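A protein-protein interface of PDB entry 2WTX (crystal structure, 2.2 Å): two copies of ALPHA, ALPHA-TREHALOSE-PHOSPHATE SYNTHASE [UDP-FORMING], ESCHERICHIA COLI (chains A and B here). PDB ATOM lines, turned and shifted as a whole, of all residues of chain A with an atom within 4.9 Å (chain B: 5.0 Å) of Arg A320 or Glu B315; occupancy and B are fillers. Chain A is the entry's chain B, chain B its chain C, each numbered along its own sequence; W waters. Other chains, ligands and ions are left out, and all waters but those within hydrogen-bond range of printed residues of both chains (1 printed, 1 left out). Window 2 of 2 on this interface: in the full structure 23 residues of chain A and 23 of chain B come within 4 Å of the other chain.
Of the 12 printed residues of chain A, 6 touch a printed residue of chain B. Printed residues of chain B that touch a printed residue of chain A: His B312, Glu B315, Asn B316, Gly B319 and Tyr B335. Hydrophobic or aromatic side chains of chain B that line the printed part of chain A: Tyr B335. Among the printed residues, 11 pairs touch across the chains. Among the printed residues, no Asp or Glu carboxylate lies within 4 Å of a Lys or Arg side-chain nitrogen of the other chain.
Water W1 lies within hydrogen-bond range of the backbone carbonyl oxygen (O) of Gly A319 (2.8 Å), the backbone carbonyl oxygen (O) of Tyr B335 (3.0 Å) and the backbone NH (N) of Gly A323 (3.2 Å).
Of chain B, only Glu B315 (3.7 Å) comes within 4 Å of Arg A320. Of the printed residues of chain A, Glu B315 touches Glu A315 (3.5 Å), Asn A316 (3.0 Å), Gly A319 (3.4 Å) and Arg A320 (3.7 Å). Printed residues of chain A within 4 Å of Gly B319: Glu A315. Of the printed residues of chain A, Tyr B335 touches Gly A319, Asn A322 and Gly A323. Of the printed residues of chain B, Asn A316 touches His B312, Glu B315 and Asn B316. Of the printed residues of chain B, Gly A323 touches Tyr B335. Printed residues of chain B within 4 Å of Glu A315: Glu B315, Asn B316 and Gly B319. Ala A318 touches none of the printed residues of chain B.
The side-chain amide oxygen of Asn A316 lies close to the side-chain amide oxygen of Asn B316, 2.8 Å away. OE1 of Glu B315 sits close to OD1 of Asn A316, at 3.0 Å.
OE1 of Glu A317 is in salt-bridge range of NH2 of Arg A320 (2.8 Å). ND1 of His B312 lies within hydrogen-bond range of OE1 of Glu B315, 3.1 Å away. NH2 of Arg B311 is in salt-bridge range of OE2 of Glu B315 (3.7 Å). The backbone carbonyl oxygen (O) of His B312 sits close to the side-chain amide oxygen (OD1) of Asn B316 (3.5 Å). The backbone carbonyl oxygen (O) of Ala A318 lies close to the side-chain amide nitrogen (ND2) of Asn A322. NH1 of Arg A320 lies within salt-bridge range of OE2 of Glu A278 (2.8 Å).
Glu A315 touches its own counterpart, Glu B315. Glu A315 touches Asn B316, and with the chains exchanged Asn A316 touches Glu B315. Glu A315 touches Gly B319, and with the chains exchanged Gly A319 touches Glu B315. Asn A316 touches its own counterpart, Asn B316. 5 positions are printed for both chains. Of the 11 pairs that touch across the chains among the printed residues, 6 have their exchanged pair printed and touching as well.
Among the printed residues, pairs that only touch across the chains: Glu A315 with Glu B315 (3.5 Å), Glu A315 with Asn B316 (3.7 Å), Glu A315 with Gly B319 (3.3 Å), Asn A316 with His B312 (3.7 Å), Gly A319 with Glu B315 (3.4 Å), Gly A319 with Tyr B335 (3.9 Å), Arg A320 with Glu B315 (3.7 Å), Asn A322 with Tyr B335 (3.8 Å) and Gly A323 with Tyr B335 (3.3 Å).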
ATOM      1  N   LEU A 275      13.863  -1.959 -10.209  1.00  0.00           N
ATOM      2  CA  LEU A 275      13.279  -0.742 -10.767  1.00  0.00           C
ATOM      3  C   LEU A 275      14.292   0.409 -10.745  1.00  0.00           C
ATOM      4  O   LEU A 275      14.305   1.236 -11.636  1.00  0.00           O
ATOM      5  CB  LEU A 275      11.989  -0.355 -10.014  1.00  0.00           C
ATOM      6  CG  LEU A 275      10.733  -1.229 -10.250  1.00  0.00           C
ATOM      7  CD1 LEU A 275       9.493  -0.708  -9.491  1.00  0.00           C
ATOM      8  CD2 LEU A 275      10.400  -1.380 -11.723  1.00  0.00           C
ATOM      9  N   GLU A 278      16.591  -0.238 -13.631  1.00  0.00           N
ATOM     10  CA  GLU A 278      15.943   0.065 -14.889  1.00  0.00           C
ATOM     11  C   GLU A 278      16.003   1.579 -15.120  1.00  0.00           C
ATOM     12  O   GLU A 278      16.295   2.030 -16.242  1.00  0.00           O
ATOM     13  CB  GLU A 278      14.513  -0.460 -14.934  1.00  0.00           C
ATOM     14  CG  GLU A 278      13.723  -0.005 -16.173  1.00  0.00           C
ATOM     15  CD  GLU A 278      12.233  -0.291 -16.094  1.00  0.00           C
ATOM     16  OE1 GLU A 278      11.638  -0.157 -14.993  1.00  0.00           O
ATOM     17  OE2 GLU A 278      11.650  -0.617 -17.152  1.00  0.00           O
ATOM     18  N   GLU A 315      11.191 -12.669 -10.658  1.00  0.00           N
ATOM     19  CA  GLU A 315      11.409 -13.371 -11.924  1.00  0.00           C
ATOM     20  C   GLU A 315      10.858 -12.608 -13.121  1.00  0.00           C
ATOM     21  O   GLU A 315      11.500 -12.551 -14.177  1.00  0.00           O
ATOM     22  CB  GLU A 315      10.706 -14.724 -11.918  1.00  0.00           C
ATOM     23  CG  GLU A 315      11.430 -15.848 -11.202  1.00  0.00           C
ATOM     24  CD  GLU A 315      10.523 -17.069 -11.002  1.00  0.00           C
ATOM     25  OE1 GLU A 315       9.369 -17.061 -11.512  1.00  0.00           O
ATOM     26  OE2 GLU A 315      10.960 -18.029 -10.335  1.00  0.00           O
ATOM     27  N   ASN A 316       9.647 -12.074 -12.956  1.00  0.00           N
ATOM     28  CA  ASN A 316       8.977 -11.301 -13.998  1.00  0.00           C
ATOM     29  C   ASN A 316       9.815 -10.069 -14.340  1.00  0.00           C
ATOM     30  O   ASN A 316      10.039  -9.769 -15.514  1.00  0.00           O
ATOM     31  CB  ASN A 316       7.556 -10.885 -13.551  1.00  0.00           C
ATOM     32  CG  ASN A 316       6.791 -10.116 -14.640  1.00  0.00           C
ATOM     33  OD1 ASN A 316       6.153 -10.714 -15.525  1.00  0.00           O
ATOM     34  ND2 ASN A 316       6.851  -8.789 -14.573  1.00  0.00           N
ATOM     35  N   GLU A 317      10.277  -9.373 -13.304  1.00  0.00           N
ATOM     36  CA  GLU A 317      11.028  -8.136 -13.475  1.00  0.00           C
ATOM     37  C   GLU A 317      12.371  -8.350 -14.178  1.00  0.00           C
ATOM     38  O   GLU A 317      12.761  -7.531 -14.993  1.00  0.00           O
ATOM     39  CB  GLU A 317      11.225  -7.416 -12.134  1.00  0.00           C
ATOM     40  CG  GLU A 317       9.971  -6.706 -11.622  1.00  0.00           C
ATOM     41  CD  GLU A 317       9.467  -5.628 -12.598  1.00  0.00           C
ATOM     42  OE1 GLU A 317      10.006  -4.507 -12.556  1.00  0.00           O
ATOM     43  OE2 GLU A 317       8.547  -5.913 -13.413  1.00  0.00           O
ATOM     44  N   ALA A 318      13.067  -9.443 -13.848  1.00  0.00           N
ATOM     45  CA  ALA A 318      14.309  -9.826 -14.552  1.00  0.00           C
ATOM     46  C   ALA A 318      14.055 -10.058 -16.042  1.00  0.00           C
ATOM     47  O   ALA A 318      14.806  -9.575 -16.886  1.00  0.00           O
ATOM     48  CB  ALA A 318      14.961 -11.084 -13.913  1.00  0.00           C
ATOM     49  N   GLY A 319      12.993 -10.792 -16.356  1.00  0.00           N
ATOM     50  CA  GLY A 319      12.666 -11.101 -17.734  1.00  0.00           C
ATOM     51  C   GLY A 319      12.293  -9.853 -18.497  1.00  0.00           C
ATOM     52  O   GLY A 319      12.724  -9.664 -19.644  1.00  0.00           O
ATOM     53  N   ARG A 320      11.519  -8.994 -17.835  1.00  0.00           N
ATOM     54  CA  ARG A 320      11.000  -7.771 -18.442  1.00  0.00           C
ATOM     55  C   ARG A 320      12.114  -6.774 -18.729  1.00  0.00           C
ATOM     56  O   ARG A 320      12.167  -6.214 -19.819  1.00  0.00           O
ATOM     57  CB  ARG A 320       9.932  -7.116 -17.545  1.00  0.00           C
ATOM     58  CG  ARG A 320       9.272  -5.860 -18.171  1.00  0.00           C
ATOM     59  CD  ARG A 320       8.315  -5.122 -17.220  1.00  0.00           C
ATOM     60  NE  ARG A 320       8.980  -4.535 -16.050  1.00  0.00           N
ATOM     61  CZ  ARG A 320       9.651  -3.385 -16.039  1.00  0.00           C
ATOM     62  NH1 ARG A 320       9.787  -2.671 -17.161  1.00  0.00           N
ATOM     63  NH2 ARG A 320      10.184  -2.938 -14.898  1.00  0.00           N
ATOM     64  N   ILE A 321      12.976  -6.532 -17.738  1.00  0.00           N
ATOM     65  CA  ILE A 321      14.030  -5.518 -17.871  1.00  0.00           C
ATOM     66  C   ILE A 321      15.085  -5.956 -18.924  1.00  0.00           C
ATOM     67  O   ILE A 321      15.481  -5.146 -19.763  1.00  0.00           O
ATOM     68  CB  ILE A 321      14.677  -5.176 -16.497  1.00  0.00           C
ATOM     69  CG1 ILE A 321      13.658  -4.487 -15.572  1.00  0.00           C
ATOM     70  CG2 ILE A 321      15.960  -4.328 -16.647  1.00  0.00           C
ATOM     71  CD1 ILE A 321      14.089  -4.447 -14.130  1.00  0.00           C
ATOM     72  N   ASN A 322      15.510  -7.222 -18.886  1.00  0.00           N
ATOM     73  CA  ASN A 322      16.398  -7.765 -19.921  1.00  0.00           C
ATOM     74  C   ASN A 322      15.758  -7.806 -21.314  1.00  0.00           C
ATOM     75  O   ASN A 322      16.439  -7.580 -22.314  1.00  0.00           O
ATOM     76  CB  ASN A 322      16.920  -9.158 -19.547  1.00  0.00           C
ATOM     77  CG  ASN A 322      18.025  -9.109 -18.494  1.00  0.00           C
ATOM     78  OD1 ASN A 322      18.792  -8.134 -18.388  1.00  0.00           O
ATOM     79  ND2 ASN A 322      18.106 -10.162 -17.707  1.00  0.00           N
ATOM     80  N   GLY A 323      14.457  -8.095 -21.356  1.00  0.00           N
ATOM     81  CA  GLY A 323      13.671  -8.075 -22.591  1.00  0.00           C
ATOM     82  C   GLY A 323      13.596  -6.695 -23.222  1.00  0.00           C
ATOM     83  O   GLY A 323      13.595  -6.551 -24.455  1.00  0.00           O
ATOM     84  N   LYS A 324      13.559  -5.676 -22.382  1.00  0.00           N
ATOM     85  CA  LYS A 324      13.411  -4.313 -22.859  1.00  0.00           C
ATOM     86  C   LYS A 324      14.763  -3.657 -23.171  1.00  0.00           C
ATOM     87  O   LYS A 324      14.888  -2.928 -24.157  1.00  0.00           O
ATOM     88  CB  LYS A 324      12.657  -3.495 -21.807  1.00  0.00           C
ATOM     89  CG  LYS A 324      12.364  -2.037 -22.197  1.00  0.00           C
ATOM     90  CD  LYS A 324      11.611  -1.333 -21.072  1.00  0.00           C
ATOM     91  CE  LYS A 324      11.473   0.167 -21.339  1.00  0.00           C
ATOM     92  NZ  LYS A 324      10.843   0.417 -22.676  1.00  0.00           N
ATOM     93  N   ARG B 311       2.758 -12.664 -23.052  1.00  0.00           N
ATOM     94  CA  ARG B 311       3.880 -11.768 -22.789  1.00  0.00           C
ATOM     95  C   ARG B 311       4.375 -11.809 -21.334  1.00  0.00           C
ATOM     96  O   ARG B 311       5.586 -11.844 -21.084  1.00  0.00           O
ATOM     97  CB  ARG B 311       3.540 -10.339 -23.194  1.00  0.00           C
ATOM     98  CG  ARG B 311       4.742  -9.404 -23.166  1.00  0.00           C
ATOM     99  CD  ARG B 311       4.398  -8.073 -23.822  1.00  0.00           C
ATOM    100  NE  ARG B 311       5.362  -7.048 -23.451  1.00  0.00           N
ATOM    101  CZ  ARG B 311       5.200  -6.200 -22.436  1.00  0.00           C
ATOM    102  NH1 ARG B 311       4.099  -6.248 -21.686  1.00  0.00           N
ATOM    103  NH2 ARG B 311       6.147  -5.303 -22.163  1.00  0.00           N
ATOM    104  N   HIS B 312       3.449 -11.822 -20.378  1.00  0.00           N
ATOM    105  CA  HIS B 312       3.864 -11.896 -18.984  1.00  0.00           C
ATOM    106  C   HIS B 312       4.458 -13.284 -18.683  1.00  0.00           C
ATOM    107  O   HIS B 312       5.429 -13.381 -17.927  1.00  0.00           O
ATOM    108  CB  HIS B 312       2.724 -11.506 -18.029  1.00  0.00           C
ATOM    109  CG  HIS B 312       2.234 -10.099 -18.219  1.00  0.00           C
ATOM    110  ND1 HIS B 312       3.081  -9.004 -18.240  1.00  0.00           N
ATOM    111  CD2 HIS B 312       0.983  -9.606 -18.391  1.00  0.00           C
ATOM    112  CE1 HIS B 312       2.369  -7.902 -18.422  1.00  0.00           C
ATOM    113  NE2 HIS B 312       1.095  -8.240 -18.515  1.00  0.00           N
ATOM    114  N   GLN B 313       3.921 -14.326 -19.320  1.00  0.00           N
ATOM    115  CA  GLN B 313       4.424 -15.691 -19.152  1.00  0.00           C
ATOM    116  C   GLN B 313       5.904 -15.811 -19.517  1.00  0.00           C
ATOM    117  O   GLN B 313       6.694 -16.414 -18.781  1.00  0.00           O
ATOM    118  CB  GLN B 313       3.597 -16.672 -19.981  1.00  0.00           C
ATOM    119  CG  GLN B 313       2.219 -16.959 -19.404  1.00  0.00           C
ATOM    120  CD  GLN B 313       1.364 -17.796 -20.337  1.00  0.00           C
ATOM    121  OE1 GLN B 313       1.876 -18.512 -21.193  1.00  0.00           O
ATOM    122  NE2 GLN B 313       0.054 -17.708 -20.170  1.00  0.00           N
ATOM    123  N   LEU B 314       6.266 -15.226 -20.660  1.00  0.00           N
ATOM    124  CA  LEU B 314       7.632 -15.233 -21.169  1.00  0.00           C
ATOM    125  C   LEU B 314       8.603 -14.454 -20.291  1.00  0.00           C
ATOM    126  O   LEU B 314       9.762 -14.870 -20.112  1.00  0.00           O
ATOM    127  CB  LEU B 314       7.653 -14.640 -22.578  1.00  0.00           C
ATOM    128  CG  LEU B 314       7.661 -15.552 -23.807  1.00  0.00           C
ATOM    129  CD1 LEU B 314       7.162 -16.993 -23.565  1.00  0.00           C
ATOM    130  CD2 LEU B 314       6.956 -14.896 -24.982  1.00  0.00           C
ATOM    131  N   GLU B 315       8.146 -13.310 -19.769  1.00  0.00           N
ATOM    132  CA  GLU B 315       8.955 -12.530 -18.825  1.00  0.00           C
ATOM    133  C   GLU B 315       9.291 -13.452 -17.653  1.00  0.00           C
ATOM    134  O   GLU B 315      10.483 -13.682 -17.352  1.00  0.00           O
ATOM    135  CB  GLU B 315       8.229 -11.252 -18.372  1.00  0.00           C
ATOM    136  CG  GLU B 315       8.054 -10.190 -19.488  1.00  0.00           C
ATOM    137  CD  GLU B 315       6.994  -9.105 -19.180  1.00  0.00           C
ATOM    138  OE1 GLU B 315       6.221  -9.236 -18.186  1.00  0.00           O
ATOM    139  OE2 GLU B 315       6.935  -8.107 -19.942  1.00  0.00           O
ATOM    140  N   ASN B 316       8.252 -14.034 -17.050  1.00  0.00           N
ATOM    141  CA  ASN B 316       8.436 -14.942 -15.919  1.00  0.00           C
ATOM    142  C   ASN B 316       9.312 -16.145 -16.243  1.00  0.00           C
ATOM    143  O   ASN B 316      10.154 -16.513 -15.452  1.00  0.00           O
ATOM    144  CB  ASN B 316       7.104 -15.372 -15.309  1.00  0.00           C
ATOM    145  CG  ASN B 316       6.633 -14.399 -14.226  1.00  0.00           C
ATOM    146  OD1 ASN B 316       6.059 -13.336 -14.520  1.00  0.00           O
ATOM    147  ND2 ASN B 316       6.926 -14.741 -12.957  1.00  0.00           N
ATOM    148  N   GLU B 317       9.144 -16.728 -17.422  1.00  0.00           N
ATOM    149  CA  GLU B 317       9.910 -17.913 -17.772  1.00  0.00           C
ATOM    150  C   GLU B 317      11.386 -17.613 -18.046  1.00  0.00           C
ATOM    151  O   GLU B 317      12.253 -18.390 -17.679  1.00  0.00           O
ATOM    152  CB  GLU B 317       9.255 -18.687 -18.915  1.00  0.00           C
ATOM    153  CG  GLU B 317       7.960 -19.414 -18.499  1.00  0.00           C
ATOM    154  CD  GLU B 317       8.171 -20.483 -17.412  1.00  0.00           C
ATOM    155  OE1 GLU B 317       8.360 -21.673 -17.775  1.00  0.00           O
ATOM    156  OE2 GLU B 317       8.160 -20.130 -16.197  1.00  0.00           O
ATOM    157  N   ALA B 318      11.660 -16.475 -18.663  1.00  0.00           N
ATOM    158  CA  ALA B 318      13.034 -16.035 -18.839  1.00  0.00           C
ATOM    159  C   ALA B 318      13.720 -15.863 -17.485  1.00  0.00           C
ATOM    160  O   ALA B 318      14.847 -16.325 -17.289  1.00  0.00           O
ATOM    161  CB  ALA B 318      13.092 -14.722 -19.643  1.00  0.00           C
ATOM    162  N   GLY B 319      13.044 -15.184 -16.557  1.00  0.00           N
ATOM    163  CA  GLY B 319      13.597 -14.938 -15.234  1.00  0.00           C
ATOM    164  C   GLY B 319      13.832 -16.241 -14.503  1.00  0.00           C
ATOM    165  O   GLY B 319      14.867 -16.422 -13.853  1.00  0.00           O
ATOM    166  N   TYR B 335      16.284 -13.367 -23.954  1.00  0.00           N
ATOM    167  CA  TYR B 335      14.965 -13.051 -24.464  1.00  0.00           C
ATOM    168  C   TYR B 335      14.869 -11.559 -24.688  1.00  0.00           C
ATOM    169  O   TYR B 335      15.116 -10.784 -23.781  1.00  0.00           O
ATOM    170  CB  TYR B 335      13.881 -13.541 -23.487  1.00  0.00           C
ATOM    171  CG  TYR B 335      12.552 -12.864 -23.662  1.00  0.00           C
ATOM    172  CD1 TYR B 335      11.772 -13.080 -24.807  1.00  0.00           C
ATOM    173  CD2 TYR B 335      12.079 -11.971 -22.698  1.00  0.00           C
ATOM    174  CE1 TYR B 335      10.526 -12.439 -24.969  1.00  0.00           C
ATOM    175  CE2 TYR B 335      10.846 -11.317 -22.853  1.00  0.00           C
ATOM    176  CZ  TYR B 335      10.077 -11.561 -23.984  1.00  0.00           C
ATOM    177  OH  TYR B 335       8.866 -10.914 -24.119  1.00  0.00           O
HETATM  178  O   HOH W   1      14.636 -11.215 -20.870  1.00  0.00           O
